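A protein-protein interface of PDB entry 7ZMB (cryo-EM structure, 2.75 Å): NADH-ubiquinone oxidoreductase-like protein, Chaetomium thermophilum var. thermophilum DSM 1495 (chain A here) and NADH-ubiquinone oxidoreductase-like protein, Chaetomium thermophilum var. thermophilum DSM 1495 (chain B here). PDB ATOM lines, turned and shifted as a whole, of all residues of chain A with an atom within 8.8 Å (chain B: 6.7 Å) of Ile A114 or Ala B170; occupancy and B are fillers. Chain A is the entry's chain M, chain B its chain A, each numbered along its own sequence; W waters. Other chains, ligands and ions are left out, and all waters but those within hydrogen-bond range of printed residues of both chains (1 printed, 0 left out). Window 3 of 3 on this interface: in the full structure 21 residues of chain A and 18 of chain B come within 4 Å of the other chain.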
ATOM      1  N   THR A 110      23.229 -11.460 -20.350  1.00  0.00           N
ATOM      2  CA  THR A 110      22.828 -10.471 -21.333  1.00  0.00           C
ATOM      3  C   THR A 110      21.565  -9.778 -20.850  1.00  0.00           C
ATOM      4  O   THR A 110      20.781 -10.349 -20.094  1.00  0.00           O
ATOM      5  CB  THR A 110      22.580 -11.111 -22.702  1.00  0.00           C
ATOM      6  OG1 THR A 110      22.169 -10.105 -23.630  1.00  0.00           O
ATOM      7  CG2 THR A 110      21.512 -12.197 -22.603  1.00  0.00           C
ATOM      8  N   HIS A 111      21.383  -8.538 -21.296  1.00  0.00           N
ATOM      9  CA  HIS A 111      20.180  -7.779 -21.007  1.00  0.00           C
ATOM     10  C   HIS A 111      19.155  -7.841 -22.130  1.00  0.00           C
ATOM     11  O   HIS A 111      17.972  -7.593 -21.883  1.00  0.00           O
ATOM     12  CB  HIS A 111      20.539  -6.320 -20.720  1.00  0.00           C
ATOM     13  CG  HIS A 111      20.900  -6.062 -19.292  1.00  0.00           C
ATOM     14  ND1 HIS A 111      19.971  -6.089 -18.275  1.00  0.00           N
ATOM     15  CD2 HIS A 111      22.090  -5.790 -18.707  1.00  0.00           C
ATOM     16  CE1 HIS A 111      20.572  -5.837 -17.127  1.00  0.00           C
ATOM     17  NE2 HIS A 111      21.858  -5.654 -17.361  1.00  0.00           N
ATOM     18  N   ASP A 112      19.573  -8.179 -23.344  1.00  0.00           N
ATOM     19  CA  ASP A 112      18.643  -8.231 -24.459  1.00  0.00           C
ATOM     20  C   ASP A 112      17.688  -9.415 -24.337  1.00  0.00           C
ATOM     21  O   ASP A 112      18.028 -10.461 -23.783  1.00  0.00           O
ATOM     22  CB  ASP A 112      19.404  -8.274 -25.789  1.00  0.00           C
ATOM     23  CG  ASP A 112      20.370  -9.439 -25.890  1.00  0.00           C
ATOM     24  OD1 ASP A 112      20.358 -10.316 -25.006  1.00  0.00           O
ATOM     25  OD2 ASP A 112      21.165  -9.473 -26.859  1.00  0.00           O
ATOM     26  N   ARG A 113      16.467  -9.219 -24.836  1.00  0.00           N
ATOM     27  CA  ARG A 113      15.469 -10.283 -24.869  1.00  0.00           C
ATOM     28  C   ARG A 113      15.945 -11.471 -25.694  1.00  0.00           C
ATOM     29  O   ARG A 113      15.671 -12.623 -25.351  1.00  0.00           O
ATOM     30  CB  ARG A 113      14.167  -9.741 -25.463  1.00  0.00           C
ATOM     31  CG  ARG A 113      13.477  -8.650 -24.682  1.00  0.00           C
ATOM     32  CD  ARG A 113      12.921  -9.163 -23.378  1.00  0.00           C
ATOM     33  NE  ARG A 113      11.938 -10.206 -23.641  1.00  0.00           N
ATOM     34  CZ  ARG A 113      10.654  -9.972 -23.891  1.00  0.00           C
ATOM     35  NH1 ARG A 113       9.824 -10.979 -24.129  1.00  0.00           N
ATOM     36  NH2 ARG A 113      10.200  -8.727 -23.920  1.00  0.00           N
ATOM     37  N   ILE A 114      16.635 -11.206 -26.799  1.00  0.00           N
ATOM     38  CA  ILE A 114      16.944 -12.205 -27.810  1.00  0.00           C
ATOM     39  C   ILE A 114      18.438 -12.159 -28.087  1.00  0.00           C
ATOM     40  O   ILE A 114      18.979 -11.091 -28.387  1.00  0.00           O
ATOM     41  CB  ILE A 114      16.138 -11.942 -29.100  1.00  0.00           C
ATOM     42  CG1 ILE A 114      14.658 -12.253 -28.883  1.00  0.00           C
ATOM     43  CG2 ILE A 114      16.703 -12.716 -30.286  1.00  0.00           C
ATOM     44  CD1 ILE A 114      13.776 -11.650 -29.913  1.00  0.00           C
ATOM     45  N   VAL A 115      19.098 -13.308 -28.009  1.00  0.00           N
ATOM     46  CA  VAL A 115      20.528 -13.403 -28.273  1.00  0.00           C
ATOM     47  C   VAL A 115      20.751 -14.179 -29.561  1.00  0.00           C
ATOM     48  O   VAL A 115      19.944 -15.024 -29.946  1.00  0.00           O
ATOM     49  CB  VAL A 115      21.293 -14.064 -27.111  1.00  0.00           C
ATOM     50  CG1 VAL A 115      21.123 -13.262 -25.881  1.00  0.00           C
ATOM     51  CG2 VAL A 115      20.806 -15.476 -26.881  1.00  0.00           C
ATOM     52  N   ALA A 116      21.861 -13.890 -30.222  1.00  0.00           N
ATOM     53  CA  ALA A 116      22.254 -14.590 -31.435  1.00  0.00           C
ATOM     54  C   ALA A 116      23.463 -15.466 -31.150  1.00  0.00           C
ATOM     55  O   ALA A 116      24.442 -15.006 -30.557  1.00  0.00           O
ATOM     56  CB  ALA A 116      22.564 -13.606 -32.562  1.00  0.00           C
ATOM     57  N   CYS A 117      23.390 -16.724 -31.562  1.00  0.00           N
ATOM     58  CA  CYS A 117      24.529 -17.625 -31.509  1.00  0.00           C
ATOM     59  C   CYS A 117      24.749 -18.218 -32.889  1.00  0.00           C
ATOM     60  O   CYS A 117      23.822 -18.762 -33.493  1.00  0.00           O
ATOM     61  CB  CYS A 117      24.331 -18.739 -30.477  1.00  0.00           C
ATOM     62  SG  CYS A 117      25.848 -19.619 -30.070  1.00  0.00           S
ATOM     63  N   LYS A 128      23.264 -19.556 -37.888  1.00  0.00           N
ATOM     64  CA  LYS A 128      22.923 -18.531 -36.913  1.00  0.00           C
ATOM     65  C   LYS A 128      21.475 -18.666 -36.469  1.00  0.00           C
ATOM     66  O   LYS A 128      20.565 -18.748 -37.294  1.00  0.00           O
ATOM     67  CB  LYS A 128      23.164 -17.145 -37.509  1.00  0.00           C
ATOM     68  CG  LYS A 128      22.943 -16.014 -36.546  1.00  0.00           C
ATOM     69  CD  LYS A 128      23.277 -14.697 -37.183  1.00  0.00           C
ATOM     70  CE  LYS A 128      23.051 -13.555 -36.218  1.00  0.00           C
ATOM     71  NZ  LYS A 128      23.370 -12.235 -36.822  1.00  0.00           N
ATOM     72  N   ILE A 129      21.259 -18.670 -35.157  1.00  0.00           N
ATOM     73  CA  ILE A 129      19.927 -18.768 -34.579  1.00  0.00           C
ATOM     74  C   ILE A 129      19.786 -17.727 -33.483  1.00  0.00           C
ATOM     75  O   ILE A 129      20.707 -16.968 -33.191  1.00  0.00           O
ATOM     76  CB  ILE A 129      19.618 -20.174 -34.024  1.00  0.00           C
ATOM     77  CG1 ILE A 129      20.601 -20.528 -32.913  1.00  0.00           C
ATOM     78  CG2 ILE A 129      19.564 -21.203 -35.150  1.00  0.00           C
ATOM     79  CD1 ILE A 129      20.237 -21.750 -32.167  1.00  0.00           C
ATOM     80  N   TYR A 130      18.609 -17.708 -32.870  1.00  0.00           N
ATOM     81  CA  TYR A 130      18.248 -16.704 -31.884  1.00  0.00           C
ATOM     82  C   TYR A 130      17.582 -17.391 -30.710  1.00  0.00           C
ATOM     83  O   TYR A 130      16.701 -18.232 -30.903  1.00  0.00           O
ATOM     84  CB  TYR A 130      17.323 -15.655 -32.499  1.00  0.00           C
ATOM     85  CG  TYR A 130      18.007 -14.888 -33.592  1.00  0.00           C
ATOM     86  CD1 TYR A 130      18.826 -13.810 -33.299  1.00  0.00           C
ATOM     87  CD2 TYR A 130      17.887 -15.281 -34.914  1.00  0.00           C
ATOM     88  CE1 TYR A 130      19.473 -13.127 -34.289  1.00  0.00           C
ATOM     89  CE2 TYR A 130      18.537 -14.608 -35.912  1.00  0.00           C
ATOM     90  CZ  TYR A 130      19.327 -13.524 -35.594  1.00  0.00           C
ATOM     91  OH  TYR A 130      19.975 -12.829 -36.579  1.00  0.00           O
ATOM     92  N   ILE A 131      17.996 -17.045 -29.498  1.00  0.00           N
ATOM     93  CA  ILE A 131      17.479 -17.683 -28.299  1.00  0.00           C
ATOM     94  C   ILE A 131      16.759 -16.627 -27.474  1.00  0.00           C
ATOM     95  O   ILE A 131      17.343 -15.600 -27.115  1.00  0.00           O
ATOM     96  CB  ILE A 131      18.585 -18.360 -27.475  1.00  0.00           C
ATOM     97  CG1 ILE A 131      19.288 -19.463 -28.265  1.00  0.00           C
ATOM     98  CG2 ILE A 131      18.000 -18.968 -26.243  1.00  0.00           C
ATOM     99  CD1 ILE A 131      20.480 -19.008 -29.043  1.00  0.00           C
ATOM    100  N   ASN A 132      15.488 -16.883 -27.186  1.00  0.00           N
ATOM    101  CA  ASN A 132      14.721 -16.066 -26.258  1.00  0.00           C
ATOM    102  C   ASN A 132      15.177 -16.344 -24.829  1.00  0.00           C
ATOM    103  O   ASN A 132      15.378 -17.498 -24.444  1.00  0.00           O
ATOM    104  CB  ASN A 132      13.232 -16.372 -26.431  1.00  0.00           C
ATOM    105  CG  ASN A 132      12.333 -15.426 -25.666  1.00  0.00           C
ATOM    106  OD1 ASN A 132      11.975 -15.686 -24.522  1.00  0.00           O
ATOM    107  ND2 ASN A 132      11.954 -14.328 -26.298  1.00  0.00           N
ATOM    108  N   THR A 133      15.368 -15.283 -24.049  1.00  0.00           N
ATOM    109  CA  THR A 133      15.714 -15.387 -22.630  1.00  0.00           C
ATOM    110  C   THR A 133      14.669 -14.618 -21.839  1.00  0.00           C
ATOM    111  O   THR A 133      14.874 -13.465 -21.466  1.00  0.00           O
ATOM    112  CB  THR A 133      17.128 -14.863 -22.344  1.00  0.00           C
ATOM    113  OG1 THR A 133      17.253 -13.522 -22.831  1.00  0.00           O
ATOM    114  CG2 THR A 133      18.174 -15.743 -22.990  1.00  0.00           C
ATOM    115  N   ASP A 134      13.565 -15.260 -21.581  1.00  0.00           N
ATOM    116  CA  ASP A 134      12.457 -14.677 -20.837  1.00  0.00           C
ATOM    117  C   ASP A 134      12.051 -15.527 -19.657  1.00  0.00           C
ATOM    118  O   ASP A 134      11.692 -14.988 -18.613  1.00  0.00           O
ATOM    119  CB  ASP A 134      11.242 -14.479 -21.730  1.00  0.00           C
ATOM    120  CG  ASP A 134      11.280 -13.187 -22.477  1.00  0.00           C
ATOM    121  OD1 ASP A 134      12.125 -12.340 -22.147  1.00  0.00           O
ATOM    122  OD2 ASP A 134      10.458 -13.013 -23.394  1.00  0.00           O
ATOM    123  N   PHE A 148      22.942 -19.236 -21.880  1.00  0.00           N
ATOM    124  CA  PHE A 148      22.629 -17.824 -21.734  1.00  0.00           C
ATOM    125  C   PHE A 148      21.596 -17.636 -20.639  1.00  0.00           C
ATOM    126  O   PHE A 148      20.742 -18.496 -20.409  1.00  0.00           O
ATOM    127  CB  PHE A 148      22.100 -17.200 -23.029  1.00  0.00           C
ATOM    128  CG  PHE A 148      22.993 -17.393 -24.200  1.00  0.00           C
ATOM    129  CD1 PHE A 148      22.914 -18.530 -24.966  1.00  0.00           C
ATOM    130  CD2 PHE A 148      23.912 -16.425 -24.546  1.00  0.00           C
ATOM    131  CE1 PHE A 148      23.748 -18.704 -26.042  1.00  0.00           C
ATOM    132  CE2 PHE A 148      24.741 -16.600 -25.627  1.00  0.00           C
ATOM    133  CZ  PHE A 148      24.655 -17.740 -26.373  1.00  0.00           C
ATOM    134  N   ASN A 150      19.294 -14.128 -18.770  1.00  0.00           N
ATOM    135  CA  ASN A 150      18.998 -12.711 -18.780  1.00  0.00           C
ATOM    136  C   ASN A 150      19.237 -12.165 -17.380  1.00  0.00           C
ATOM    137  O   ASN A 150      18.872 -12.797 -16.387  1.00  0.00           O
ATOM    138  CB  ASN A 150      17.563 -12.455 -19.235  1.00  0.00           C
ATOM    139  CG  ASN A 150      17.277 -10.988 -19.469  1.00  0.00           C
ATOM    140  OD1 ASN A 150      18.135 -10.135 -19.272  1.00  0.00           O
ATOM    141  ND2 ASN A 150      16.065 -10.687 -19.899  1.00  0.00           N
ATOM    142  N   ASN B 132      11.482 -14.571 -40.398  1.00  0.00           N
ATOM    143  CA  ASN B 132      11.793 -14.751 -38.962  1.00  0.00           C
ATOM    144  C   ASN B 132      11.767 -16.231 -38.622  1.00  0.00           C
ATOM    145  O   ASN B 132      11.859 -16.554 -37.443  1.00  0.00           O
ATOM    146  CB  ASN B 132      10.928 -13.890 -38.042  1.00  0.00           C
ATOM    147  CG  ASN B 132      11.170 -12.408 -38.163  1.00  0.00           C
ATOM    148  OD1 ASN B 132      12.289 -11.965 -38.400  1.00  0.00           O
ATOM    149  ND2 ASN B 132      10.117 -11.639 -37.971  1.00  0.00           N
ATOM    150  N   GLY B 166      19.273  -6.441 -36.761  1.00  0.00           N
ATOM    151  CA  GLY B 166      18.364  -6.629 -35.646  1.00  0.00           C
ATOM    152  C   GLY B 166      18.034  -8.076 -35.354  1.00  0.00           C
ATOM    153  O   GLY B 166      17.608  -8.390 -34.240  1.00  0.00           O
ATOM    154  N   GLY B 167      18.218  -8.960 -36.319  1.00  0.00           N
ATOM    155  CA  GLY B 167      17.962 -10.365 -36.107  1.00  0.00           C
ATOM    156  C   GLY B 167      16.513 -10.745 -36.326  1.00  0.00           C
ATOM    157  O   GLY B 167      15.665  -9.950 -36.732  1.00  0.00           O
ATOM    158  N   LYS B 168      16.235 -12.006 -36.033  1.00  0.00           N
ATOM    159  CA  LYS B 168      14.914 -12.584 -36.196  1.00  0.00           C
ATOM    160  C   LYS B 168      14.142 -12.526 -34.887  1.00  0.00           C
ATOM    161  O   LYS B 168      14.687 -12.241 -33.824  1.00  0.00           O
ATOM    162  CB  LYS B 168      15.022 -14.030 -36.683  1.00  0.00           C
ATOM    163  CG  LYS B 168      15.642 -14.203 -38.038  1.00  0.00           C
ATOM    164  CD  LYS B 168      15.695 -15.669 -38.402  1.00  0.00           C
ATOM    165  CE  LYS B 168      16.387 -15.908 -39.727  1.00  0.00           C
ATOM    166  NZ  LYS B 168      15.450 -15.935 -40.871  1.00  0.00           N
ATOM    167  N   ARG B 169      12.849 -12.806 -34.983  1.00  0.00           N
ATOM    168  CA  ARG B 169      12.016 -12.954 -33.801  1.00  0.00           C
ATOM    169  C   ARG B 169      12.324 -14.264 -33.095  1.00  0.00           C
ATOM    170  O   ARG B 169      12.462 -15.312 -33.727  1.00  0.00           O
ATOM    171  CB  ARG B 169      10.540 -12.908 -34.190  1.00  0.00           C
ATOM    172  CG  ARG B 169       9.643 -13.791 -33.344  1.00  0.00           C
ATOM    173  CD  ARG B 169       8.382 -14.144 -34.072  1.00  0.00           C
ATOM    174  NE  ARG B 169       8.651 -14.960 -35.247  1.00  0.00           N
ATOM    175  CZ  ARG B 169       7.818 -15.095 -36.271  1.00  0.00           C
ATOM    176  NH1 ARG B 169       6.650 -14.471 -36.274  1.00  0.00           N
ATOM    177  NH2 ARG B 169       8.160 -15.861 -37.291  1.00  0.00           N
ATOM    178  N   ALA B 170      12.443 -14.204 -31.780  1.00  0.00           N
ATOM    179  CA  ALA B 170      12.570 -15.397 -30.960  1.00  0.00           C
ATOM    180  C   ALA B 170      11.519 -15.352 -29.862  1.00  0.00           C
ATOM    181  O   ALA B 170      11.324 -14.315 -29.227  1.00  0.00           O
ATOM    182  CB  ALA B 170      13.966 -15.512 -30.363  1.00  0.00           C
ATOM    183  N   VAL B 171      10.823 -16.468 -29.659  1.00  0.00           N
ATOM    184  CA  VAL B 171       9.827 -16.585 -28.605  1.00  0.00           C
ATOM    185  C   VAL B 171      10.181 -17.777 -27.731  1.00  0.00           C
ATOM    186  O   VAL B 171      10.913 -18.679 -28.135  1.00  0.00           O
ATOM    187  CB  VAL B 171       8.381 -16.714 -29.143  1.00  0.00           C
ATOM    188  CG1 VAL B 171       7.968 -15.450 -29.856  1.00  0.00           C
ATOM    189  CG2 VAL B 171       8.251 -17.896 -30.073  1.00  0.00           C
ATOM    190  N   GLU B 172       9.654 -17.763 -26.512  1.00  0.00           N
ATOM    191  CA  GLU B 172       9.992 -18.778 -25.531  1.00  0.00           C
ATOM    192  C   GLU B 172       9.154 -20.029 -25.745  1.00  0.00           C
ATOM    193  O   GLU B 172       8.067 -19.984 -26.324  1.00  0.00           O
ATOM    194  CB  GLU B 172       9.777 -18.241 -24.119  1.00  0.00           C
ATOM    195  CG  GLU B 172       8.334 -18.020 -23.755  1.00  0.00           C
ATOM    196  CD  GLU B 172       7.811 -16.681 -24.215  1.00  0.00           C
ATOM    197  OE1 GLU B 172       8.455 -16.036 -25.070  1.00  0.00           O
ATOM    198  OE2 GLU B 172       6.746 -16.267 -23.718  1.00  0.00           O
ATOM    199  N   ASN B 185       9.727 -21.012 -32.113  1.00  0.00           N
ATOM    200  CA  ASN B 185      10.339 -20.075 -33.082  1.00  0.00           C
ATOM    201  C   ASN B 185       9.850 -20.514 -34.462  1.00  0.00           C
ATOM    202  O   ASN B 185       9.641 -19.671 -35.309  1.00  0.00           O
ATOM    203  CB  ASN B 185      11.868 -19.953 -32.970  1.00  0.00           C
ATOM    204  CG  ASN B 185      12.360 -19.298 -31.703  1.00  0.00           C
ATOM    205  OD1 ASN B 185      11.571 -18.807 -30.911  1.00  0.00           O
ATOM    206  ND2 ASN B 185      13.666 -19.285 -31.508  1.00  0.00           N
ATOM    207  N   ASP B 214       4.334 -10.410 -32.403  1.00  0.00           N
ATOM    208  CA  ASP B 214       4.492 -11.111 -31.140  1.00  0.00           C
ATOM    209  C   ASP B 214       3.292 -11.993 -30.799  1.00  0.00           C
ATOM    210  O   ASP B 214       3.185 -12.464 -29.667  1.00  0.00           O
ATOM    211  CB  ASP B 214       4.750 -10.110 -30.015  1.00  0.00           C
ATOM    212  CG  ASP B 214       5.581 -10.699 -28.899  1.00  0.00           C
ATOM    213  OD1 ASP B 214       6.484 -11.510 -29.198  1.00  0.00           O
ATOM    214  OD2 ASP B 214       5.342 -10.355 -27.724  1.00  0.00           O
HETATM  215  O   HOH W   1      14.228 -19.348 -28.200  1.00  0.00           O
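Among the printed residues, merely in contact across the chains: Tyr A130 with Gly B167 (3.2 Å), Asn A132 with Glu B172 (3.4 Å), Ile A114 with Ala B170 (3.4 Å), Tyr A130 with Lys B168 (3.5 Å), Asn A132 with Val B171 (3.6 Å), Tyr A130 with Ala B170 (3.9 Å) and Asp A134 with Glu B172 (3.99 Å).
Water W1 lies within hydrogen-bond range of the backbone NH of Asn A132 (2.9 Å), the side-chain amide nitrogen of Asn B185 (3.4 Å) and the backbone carbonyl oxygen of Val B171 (3.4 Å).
Of the 10 printed residues of chain B, 6 touch a printed residue of chain A.
Printed residues of chain B that touch a printed residue of chain A: Gly B167, Lys B168, Ala B170, Val B171, Glu B172 and Asn B185.
Hydrophobic or aromatic side chains of chain B within 4 Å of the printed part of chain A: Ala B170.
Of the 17 printed residues of chain A, 4 touch a printed residue of chain B.
OD1 of Asn A132 lies close to OD2 of Asp A134 (3.3 Å).
N of Val B171 lies within hydrogen-bond range of OD1 of Asn B185.
OD1 of Asp A134 lies within salt-bridge range of NE of Arg A113, 2.6 Å away.
The side-chain hydroxyl (OH) of Tyr A130 sits close to the side-chain amino group (NZ) of Lys A128 (3.5 Å).
The side-chain amide nitrogen of Asn A132 sits at hydrogen-bond distance from the backbone carbonyl oxygen of Ala B170 (3.0 Å).
The backbone carbonyl oxygen (O) of Tyr A130 sits at hydrogen-bond distance from the side-chain amide nitrogen (ND2) of Asn B185 (3.3 Å).
Of the printed residues of chain B, Ile A114 touches Ala B170 (3.4 Å).
Printed residues of chain B within 4 Å of Asn A132: Ala B170 (3.0 Å), Val B171 (3.6 Å) and Glu B172 (3.4 Å).
Of the printed residues of chain A, Lys B168 touches Tyr A130.
Ala B170 touches three residues of chain A.
Val B171 touches one residue of chain A.
Of the printed residues of chain A, Asn B185 touches Tyr A130 (3.3 Å).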
